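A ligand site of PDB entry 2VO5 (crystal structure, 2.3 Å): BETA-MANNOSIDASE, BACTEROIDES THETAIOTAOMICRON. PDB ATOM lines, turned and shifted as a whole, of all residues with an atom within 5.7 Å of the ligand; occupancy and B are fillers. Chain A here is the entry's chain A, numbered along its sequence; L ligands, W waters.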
ATOM      1  N   ASN A 153     -27.570  11.067 -10.416  1.00  0.00           N
ATOM      2  CA  ASN A 153     -27.479  10.952 -11.883  1.00  0.00           C
ATOM      3  C   ASN A 153     -28.519  10.017 -12.458  1.00  0.00           C
ATOM      4  O   ASN A 153     -28.698  10.001 -13.636  1.00  0.00           O
ATOM      5  CB  ASN A 153     -26.074  10.551 -12.348  1.00  0.00           C
ATOM      6  CG  ASN A 153     -25.032  11.644 -12.167  1.00  0.00           C
ATOM      7  OD1 ASN A 153     -24.986  12.608 -12.939  1.00  0.00           O
ATOM      8  ND2 ASN A 153     -24.188  11.509 -11.146  1.00  0.00           N
ATOM      9  N   TRP A 173     -27.442  10.750 -16.740  1.00  0.00           N
ATOM     10  CA  TRP A 173     -26.147  11.292 -16.221  1.00  0.00           C
ATOM     11  C   TRP A 173     -25.984  12.786 -16.568  1.00  0.00           C
ATOM     12  O   TRP A 173     -26.742  13.281 -17.385  1.00  0.00           O
ATOM     13  CB  TRP A 173     -24.924  10.449 -16.687  1.00  0.00           C
ATOM     14  CG  TRP A 173     -23.901  10.282 -15.550  1.00  0.00           C
ATOM     15  CD1 TRP A 173     -22.896  11.124 -15.248  1.00  0.00           C
ATOM     16  CD2 TRP A 173     -23.850   9.227 -14.562  1.00  0.00           C
ATOM     17  NE1 TRP A 173     -22.186  10.669 -14.171  1.00  0.00           N
ATOM     18  CE2 TRP A 173     -22.770   9.512 -13.715  1.00  0.00           C
ATOM     19  CE3 TRP A 173     -24.589   8.050 -14.340  1.00  0.00           C
ATOM     20  CZ2 TRP A 173     -22.429   8.685 -12.618  1.00  0.00           C
ATOM     21  CZ3 TRP A 173     -24.246   7.231 -13.279  1.00  0.00           C
ATOM     22  CH2 TRP A 173     -23.164   7.550 -12.430  1.00  0.00           C
ATOM     23  N   ASP A 174     -24.999  13.507 -16.014  1.00  0.00           N
ATOM     24  CA  ASP A 174     -24.887  14.983 -16.259  1.00  0.00           C
ATOM     25  C   ASP A 174     -24.342  15.342 -17.637  1.00  0.00           C
ATOM     26  O   ASP A 174     -24.041  16.502 -17.917  1.00  0.00           O
ATOM     27  CB  ASP A 174     -24.151  15.752 -15.152  1.00  0.00           C
ATOM     28  CG  ASP A 174     -22.809  15.155 -14.785  1.00  0.00           C
ATOM     29  OD1 ASP A 174     -22.176  14.445 -15.617  1.00  0.00           O
ATOM     30  OD2 ASP A 174     -22.389  15.372 -13.622  1.00  0.00           O
ATOM     31  N   TRP A 175     -24.246  14.345 -18.503  1.00  0.00           N
ATOM     32  CA  TRP A 175     -23.893  14.579 -19.884  1.00  0.00           C
ATOM     33  C   TRP A 175     -24.712  13.631 -20.764  1.00  0.00           C
ATOM     34  O   TRP A 175     -24.470  13.526 -21.978  1.00  0.00           O
ATOM     35  CB  TRP A 175     -22.385  14.355 -20.074  1.00  0.00           C
ATOM     36  CG  TRP A 175     -21.828  13.168 -19.264  1.00  0.00           C
ATOM     37  CD1 TRP A 175     -21.016  13.256 -18.182  1.00  0.00           C
ATOM     38  CD2 TRP A 175     -22.046  11.760 -19.496  1.00  0.00           C
ATOM     39  NE1 TRP A 175     -20.704  12.000 -17.724  1.00  0.00           N
ATOM     40  CE2 TRP A 175     -21.337  11.064 -18.503  1.00  0.00           C
ATOM     41  CE3 TRP A 175     -22.787  11.029 -20.447  1.00  0.00           C
ATOM     42  CZ2 TRP A 175     -21.319   9.656 -18.423  1.00  0.00           C
ATOM     43  CZ3 TRP A 175     -22.797   9.647 -20.365  1.00  0.00           C
ATOM     44  CH2 TRP A 175     -22.062   8.972 -19.354  1.00  0.00           C
ATOM     45  N   ARG A 368      -8.944   5.883 -19.117  1.00  0.00           N
ATOM     46  CA  ARG A 368      -9.716   5.384 -17.994  1.00  0.00           C
ATOM     47  C   ARG A 368     -11.122   5.008 -18.493  1.00  0.00           C
ATOM     48  O   ARG A 368     -11.879   5.874 -19.049  1.00  0.00           O
ATOM     49  CB  ARG A 368      -9.772   6.444 -16.863  1.00  0.00           C
ATOM     50  CG  ARG A 368     -10.585   6.013 -15.646  1.00  0.00           C
ATOM     51  CD  ARG A 368     -10.457   6.963 -14.445  1.00  0.00           C
ATOM     52  NE  ARG A 368     -11.452   6.626 -13.432  1.00  0.00           N
ATOM     53  CZ  ARG A 368     -12.263   7.496 -12.839  1.00  0.00           C
ATOM     54  NH1 ARG A 368     -12.140   8.801 -13.112  1.00  0.00           N
ATOM     55  NH2 ARG A 368     -13.171   7.083 -11.955  1.00  0.00           N
ATOM     56  N   TRP A 370     -14.270   4.543 -17.151  1.00  0.00           N
ATOM     57  CA  TRP A 370     -14.909   5.070 -15.940  1.00  0.00           C
ATOM     58  C   TRP A 370     -16.115   4.254 -15.541  1.00  0.00           C
ATOM     59  O   TRP A 370     -16.800   3.666 -16.389  1.00  0.00           O
ATOM     60  CB  TRP A 370     -15.267   6.535 -16.227  1.00  0.00           C
ATOM     61  CG  TRP A 370     -16.303   7.167 -15.436  1.00  0.00           C
ATOM     62  CD1 TRP A 370     -16.122   7.889 -14.294  1.00  0.00           C
ATOM     63  CD2 TRP A 370     -17.709   7.257 -15.758  1.00  0.00           C
ATOM     64  NE1 TRP A 370     -17.341   8.389 -13.857  1.00  0.00           N
ATOM     65  CE2 TRP A 370     -18.322   8.020 -14.740  1.00  0.00           C
ATOM     66  CE3 TRP A 370     -18.512   6.725 -16.799  1.00  0.00           C
ATOM     67  CZ2 TRP A 370     -19.681   8.281 -14.726  1.00  0.00           C
ATOM     68  CZ3 TRP A 370     -19.844   6.961 -16.787  1.00  0.00           C
ATOM     69  CH2 TRP A 370     -20.438   7.758 -15.750  1.00  0.00           C
ATOM     70  N   ALA A 398     -20.344   4.043  -9.513  1.00  0.00           N
ATOM     71  CA  ALA A 398     -20.055   5.486  -9.658  1.00  0.00           C
ATOM     72  C   ALA A 398     -21.052   6.411  -8.879  1.00  0.00           C
ATOM     73  O   ALA A 398     -22.278   6.214  -8.904  1.00  0.00           O
ATOM     74  CB  ALA A 398     -20.038   5.876 -11.138  1.00  0.00           C
ATOM     75  N   CYS A 399     -20.470   7.351  -8.157  1.00  0.00           N
ATOM     76  CA  CYS A 399     -21.104   8.548  -7.622  1.00  0.00           C
ATOM     77  C   CYS A 399     -22.096   8.373  -6.489  1.00  0.00           C
ATOM     78  O   CYS A 399     -22.628   9.375  -5.982  1.00  0.00           O
ATOM     79  CB  CYS A 399     -21.661   9.436  -8.758  1.00  0.00           C
ATOM     80  SG  CYS A 399     -20.357  10.130  -9.810  1.00  0.00           S
ATOM     81  N   ASN A 436     -15.884   4.989  -8.912  1.00  0.00           N
ATOM     82  CA  ASN A 436     -15.734   6.405  -9.122  1.00  0.00           C
ATOM     83  C   ASN A 436     -16.403   7.227  -8.013  1.00  0.00           C
ATOM     84  O   ASN A 436     -17.637   7.228  -7.895  1.00  0.00           O
ATOM     85  CB  ASN A 436     -16.370   6.785 -10.467  1.00  0.00           C
ATOM     86  CG  ASN A 436     -16.245   8.228 -10.758  1.00  0.00           C
ATOM     87  OD1 ASN A 436     -15.145   8.708 -10.955  1.00  0.00           O
ATOM     88  ND2 ASN A 436     -17.359   8.948 -10.765  1.00  0.00           N
ATOM     89  N   GLU A 437     -15.590   7.923  -7.198  1.00  0.00           N
ATOM     90  CA  GLU A 437     -16.077   9.024  -6.349  1.00  0.00           C
ATOM     91  C   GLU A 437     -17.042   8.647  -5.214  1.00  0.00           C
ATOM     92  O   GLU A 437     -17.644   9.509  -4.609  1.00  0.00           O
ATOM     93  CB  GLU A 437     -16.690  10.117  -7.225  1.00  0.00           C
ATOM     94  CG  GLU A 437     -15.724  11.051  -7.897  1.00  0.00           C
ATOM     95  CD  GLU A 437     -16.416  12.021  -8.845  1.00  0.00           C
ATOM     96  OE1 GLU A 437     -17.663  11.924  -8.999  1.00  0.00           O
ATOM     97  OE2 GLU A 437     -15.726  12.856  -9.470  1.00  0.00           O
ATOM     98  N   TRP A 445     -20.258  14.782   0.519  1.00  0.00           N
ATOM     99  CA  TRP A 445     -21.418  15.264  -0.251  1.00  0.00           C
ATOM    100  C   TRP A 445     -22.658  15.499   0.626  1.00  0.00           C
ATOM    101  O   TRP A 445     -23.780  15.635   0.125  1.00  0.00           O
ATOM    102  CB  TRP A 445     -21.719  14.421  -1.501  1.00  0.00           C
ATOM    103  CG  TRP A 445     -20.615  14.448  -2.562  1.00  0.00           C
ATOM    104  CD1 TRP A 445     -19.502  15.233  -2.547  1.00  0.00           C
ATOM    105  CD2 TRP A 445     -20.539  13.670  -3.784  1.00  0.00           C
ATOM    106  NE1 TRP A 445     -18.739  14.998  -3.666  1.00  0.00           N
ATOM    107  CE2 TRP A 445     -19.343  14.045  -4.442  1.00  0.00           C
ATOM    108  CE3 TRP A 445     -21.354  12.678  -4.369  1.00  0.00           C
ATOM    109  CZ2 TRP A 445     -18.951  13.475  -5.668  1.00  0.00           C
ATOM    110  CZ3 TRP A 445     -20.962  12.109  -5.594  1.00  0.00           C
ATOM    111  CH2 TRP A 445     -19.754  12.499  -6.220  1.00  0.00           C
ATOM    112  N   HIS A 506      -9.298  14.324  -8.537  1.00  0.00           N
ATOM    113  CA  HIS A 506     -10.279  14.860  -9.478  1.00  0.00           C
ATOM    114  C   HIS A 506     -10.383  16.393  -9.235  1.00  0.00           C
ATOM    115  O   HIS A 506     -11.113  16.844  -8.355  1.00  0.00           O
ATOM    116  CB  HIS A 506     -11.679  14.228  -9.237  1.00  0.00           C
ATOM    117  CG  HIS A 506     -11.770  12.767  -9.564  1.00  0.00           C
ATOM    118  ND1 HIS A 506     -12.972  12.095  -9.635  1.00  0.00           N
ATOM    119  CD2 HIS A 506     -10.809  11.843  -9.835  1.00  0.00           C
ATOM    120  CE1 HIS A 506     -12.758  10.821  -9.928  1.00  0.00           C
ATOM    121  NE2 HIS A 506     -11.455  10.648 -10.064  1.00  0.00           N
ATOM    122  N   TRP A 508     -11.941  19.310  -9.532  1.00  0.00           N
ATOM    123  CA  TRP A 508     -13.143  20.005  -9.957  1.00  0.00           C
ATOM    124  C   TRP A 508     -13.300  21.431  -9.398  1.00  0.00           C
ATOM    125  O   TRP A 508     -14.405  21.966  -9.326  1.00  0.00           O
ATOM    126  CB  TRP A 508     -14.401  19.112  -9.796  1.00  0.00           C
ATOM    127  CG  TRP A 508     -14.406  18.027 -10.852  1.00  0.00           C
ATOM    128  CD1 TRP A 508     -14.122  16.722 -10.683  1.00  0.00           C
ATOM    129  CD2 TRP A 508     -14.651  18.206 -12.254  1.00  0.00           C
ATOM    130  NE1 TRP A 508     -14.158  16.060 -11.881  1.00  0.00           N
ATOM    131  CE2 TRP A 508     -14.496  16.938 -12.866  1.00  0.00           C
ATOM    132  CE3 TRP A 508     -14.968  19.329 -13.063  1.00  0.00           C
ATOM    133  CZ2 TRP A 508     -14.673  16.745 -14.241  1.00  0.00           C
ATOM    134  CZ3 TRP A 508     -15.129  19.145 -14.418  1.00  0.00           C
ATOM    135  CH2 TRP A 508     -14.986  17.846 -15.014  1.00  0.00           C
ATOM    136  N   TYR A 512     -16.778  23.272 -11.467  1.00  0.00           N
ATOM    137  CA  TYR A 512     -17.578  23.281 -10.230  1.00  0.00           C
ATOM    138  C   TYR A 512     -17.203  24.322  -9.177  1.00  0.00           C
ATOM    139  O   TYR A 512     -18.056  24.762  -8.455  1.00  0.00           O
ATOM    140  CB  TYR A 512     -17.677  21.879  -9.555  1.00  0.00           C
ATOM    141  CG  TYR A 512     -18.395  20.945 -10.439  1.00  0.00           C
ATOM    142  CD1 TYR A 512     -19.783  21.030 -10.576  1.00  0.00           C
ATOM    143  CD2 TYR A 512     -17.688  20.026 -11.247  1.00  0.00           C
ATOM    144  CE1 TYR A 512     -20.465  20.211 -11.487  1.00  0.00           C
ATOM    145  CE2 TYR A 512     -18.369  19.175 -12.144  1.00  0.00           C
ATOM    146  CZ  TYR A 512     -19.761  19.290 -12.271  1.00  0.00           C
ATOM    147  OH  TYR A 512     -20.438  18.490 -13.155  1.00  0.00           O
ATOM    148  N   GLU A 530      -8.949  13.274 -13.058  1.00  0.00           N
ATOM    149  CA  GLU A 530     -10.012  14.024 -13.730  1.00  0.00           C
ATOM    150  C   GLU A 530      -9.846  15.508 -13.538  1.00  0.00           C
ATOM    151  O   GLU A 530      -9.539  15.936 -12.436  1.00  0.00           O
ATOM    152  CB  GLU A 530     -11.387  13.665 -13.182  1.00  0.00           C
ATOM    153  CG  GLU A 530     -11.930  12.259 -13.490  1.00  0.00           C
ATOM    154  CD  GLU A 530     -13.334  12.084 -12.953  1.00  0.00           C
ATOM    155  OE1 GLU A 530     -13.922  13.120 -12.652  1.00  0.00           O
ATOM    156  OE2 GLU A 530     -13.865  10.945 -12.841  1.00  0.00           O
ATOM    157  N   SER A 564     -25.855  19.475 -17.193  1.00  0.00           N
ATOM    158  CA  SER A 564     -25.409  20.314 -16.086  1.00  0.00           C
ATOM    159  C   SER A 564     -26.419  21.483 -16.087  1.00  0.00           C
ATOM    160  O   SER A 564     -26.587  22.203 -17.095  1.00  0.00           O
ATOM    161  CB  SER A 564     -23.955  20.783 -16.298  1.00  0.00           C
ATOM    162  OG  SER A 564     -23.148  20.476 -15.135  1.00  0.00           O
ATOM    163  N   TRP A 620     -11.227  14.809 -18.122  1.00  0.00           N
ATOM    164  CA  TRP A 620     -12.624  14.560 -18.283  1.00  0.00           C
ATOM    165  C   TRP A 620     -13.203  15.461 -19.417  1.00  0.00           C
ATOM    166  O   TRP A 620     -13.289  16.667 -19.213  1.00  0.00           O
ATOM    167  CB  TRP A 620     -13.362  14.835 -16.936  1.00  0.00           C
ATOM    168  CG  TRP A 620     -14.779  14.359 -17.122  1.00  0.00           C
ATOM    169  CD1 TRP A 620     -15.854  15.089 -17.615  1.00  0.00           C
ATOM    170  CD2 TRP A 620     -15.227  12.992 -17.014  1.00  0.00           C
ATOM    171  NE1 TRP A 620     -16.963  14.249 -17.737  1.00  0.00           N
ATOM    172  CE2 TRP A 620     -16.586  12.970 -17.374  1.00  0.00           C
ATOM    173  CE3 TRP A 620     -14.616  11.798 -16.585  1.00  0.00           C
ATOM    174  CZ2 TRP A 620     -17.335  11.778 -17.325  1.00  0.00           C
ATOM    175  CZ3 TRP A 620     -15.355  10.636 -16.570  1.00  0.00           C
ATOM    176  CH2 TRP A 620     -16.692  10.641 -16.941  1.00  0.00           C
ATOM    177  N   GLN A 621     -13.676  14.952 -20.565  1.00  0.00           N
ATOM    178  CA  GLN A 621     -13.884  13.548 -20.927  1.00  0.00           C
ATOM    179  C   GLN A 621     -13.503  13.435 -22.417  1.00  0.00           C
ATOM    180  O   GLN A 621     -13.490  14.438 -23.129  1.00  0.00           O
ATOM    181  CB  GLN A 621     -15.353  13.136 -20.730  1.00  0.00           C
ATOM    182  CG  GLN A 621     -16.374  13.786 -21.738  1.00  0.00           C
ATOM    183  CD  GLN A 621     -17.807  13.820 -21.215  1.00  0.00           C
ATOM    184  OE1 GLN A 621     -18.163  14.679 -20.376  1.00  0.00           O
ATOM    185  NE2 GLN A 621     -18.655  12.916 -21.703  1.00  0.00           N
ATOM    186  N   TRP A 631     -18.254  18.155 -21.485  1.00  0.00           N
ATOM    187  CA  TRP A 631     -16.822  18.278 -21.296  1.00  0.00           C
ATOM    188  C   TRP A 631     -15.952  17.564 -22.331  1.00  0.00           C
ATOM    189  O   TRP A 631     -14.727  17.608 -22.223  1.00  0.00           O
ATOM    190  CB  TRP A 631     -16.477  17.719 -19.940  1.00  0.00           C
ATOM    191  CG  TRP A 631     -17.167  18.370 -18.773  1.00  0.00           C
ATOM    192  CD1 TRP A 631     -16.627  19.281 -17.931  1.00  0.00           C
ATOM    193  CD2 TRP A 631     -18.504  18.118 -18.298  1.00  0.00           C
ATOM    194  NE1 TRP A 631     -17.527  19.627 -16.954  1.00  0.00           N
ATOM    195  CE2 TRP A 631     -18.699  18.937 -17.162  1.00  0.00           C
ATOM    196  CE3 TRP A 631     -19.552  17.269 -18.697  1.00  0.00           C
ATOM    197  CZ2 TRP A 631     -19.902  18.942 -16.418  1.00  0.00           C
ATOM    198  CZ3 TRP A 631     -20.765  17.269 -17.963  1.00  0.00           C
ATOM    199  CH2 TRP A 631     -20.926  18.113 -16.858  1.00  0.00           C
HETATM  200  O1  LIG L   1     -16.489  11.154 -12.349  1.00  0.00           O
HETATM  201  C1  LIG L   1     -17.020  12.219 -13.135  1.00  0.00           C
HETATM  202  C2  LIG L   1     -18.372  11.855 -13.708  1.00  0.00           C
HETATM  203  O2  LIG L   1     -18.931  10.882 -12.874  1.00  0.00           O
HETATM  204  C3  LIG L   1     -19.177  13.156 -13.719  1.00  0.00           C
HETATM  205  O3  LIG L   1     -20.371  12.947 -14.532  1.00  0.00           O
HETATM  206  C4  LIG L   1     -18.297  14.237 -14.386  1.00  0.00           C
HETATM  207  C5  LIG L   1     -19.015  15.436 -15.022  1.00  0.00           C
HETATM  208  O4  LIG L   1     -19.538  16.247 -13.985  1.00  0.00           O
HETATM  209  C6  LIG L   1     -17.175  14.650 -13.428  1.00  0.00           C
HETATM  210  C7  LIG L   1     -19.562  13.516 -12.273  1.00  0.00           C
HETATM  211  N1  LIG L   1     -18.322  13.694 -11.475  1.00  0.00           N
HETATM  212  C8  LIG L   1     -17.137  13.556 -12.370  1.00  0.00           C
HETATM  213  C9  LIG L   1     -18.231  15.005 -10.750  1.00  0.00           C
HETATM  214  C10 LIG L   1     -19.434  15.396  -9.908  1.00  0.00           C
HETATM  215  C11 LIG L   1     -19.912  14.573  -8.888  1.00  0.00           C
HETATM  216  C12 LIG L   1     -21.032  14.960  -8.117  1.00  0.00           C
HETATM  217  C13 LIG L   1     -20.122  16.598 -10.174  1.00  0.00           C
HETATM  218  C14 LIG L   1     -21.245  16.983  -9.420  1.00  0.00           C
HETATM  219  C15 LIG L   1     -21.698  16.157  -8.379  1.00  0.00           C
HETATM  220  O   HOH W   1     -22.781  14.357 -11.264  1.00  0.00           O
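O4 of the ligand is in hydrogen-bond range of OH of Tyr 512, 2.6 Å away. OD1 of Asp 174 lies within hydrogen-bond range of O3 of the ligand. OE2 of Glu 530 lies within hydrogen-bond range of O1 of the ligand (2.7 Å). The side-chain amide nitrogen (ND2) of Asn 436 is in hydrogen-bond range of an oxygen (O1) of the ligand (2.9 Å). NE1 of Trp 173 sits at hydrogen-bond distance from O3 of the ligand, at 2.9 Å. N1 of the ligand lies within salt-bridge range of OE1 of Glu 437, at 3.1 Å. O2 of the ligand is in hydrogen-bond range of NE1 of Trp 370, 3.1 Å away. NE1 of Trp 175 lies within hydrogen-bond range of O3 of the ligand. The side-chain sulfur (SG) of Cys 399 lies within hydrogen-bond range of an oxygen (O2) of the ligand (3.5 Å).
The backbone NH (N) of Asp 174 sits at hydrogen-bond distance from the side-chain amide oxygen (OD1) of Asn 153, at 3.2 Å. ND2 of Asn 436 sits at hydrogen-bond distance from OE1 of Glu 437, 3.5 Å away. The backbone NH (N) of Cys 399 is in hydrogen-bond range of the backbone carbonyl oxygen (O) of Asn 436. NH2 of Arg 368 sits at hydrogen-bond distance from OD1 of Asn 436 (2.7 Å). The backbone carbonyl oxygen (O) of Asn 153 is in hydrogen-bond range of the backbone NH (N) of Trp 173, 3.4 Å away. OE1 of Glu 437 sits at hydrogen-bond distance from SG of Cys 399 (3.3 Å). OE2 of Glu 437 is in hydrogen-bond range of ND1 of His 506 (2.9 Å). NE1 of Trp 620 is in hydrogen-bond range of OE1 of Gln 621, 2.9 Å away.
Trp 445 touches the ligand (CH2 to C12, 3.4 Å). Trp 508 touches the ligand. Trp 620 touches the ligand. Trp 631 touches the ligand. 13 residues have an atom within 4 Å of the ligand: Trp 173, Asp 174, Trp 175, Trp 370, Cys 399, Asn 436, Glu 437, Trp 445, Trp 508, Tyr 512, Glu 530, Trp 620 and Trp 631. The nearest printed residue that does not touch the ligand is His 506 (4.5 Å).
Water W1 lies within hydrogen-bond range of the side-chain carboxylate of Asp 174 (2.6 Å) and the side-chain amide nitrogen of Asn 153 (3.2 Å).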
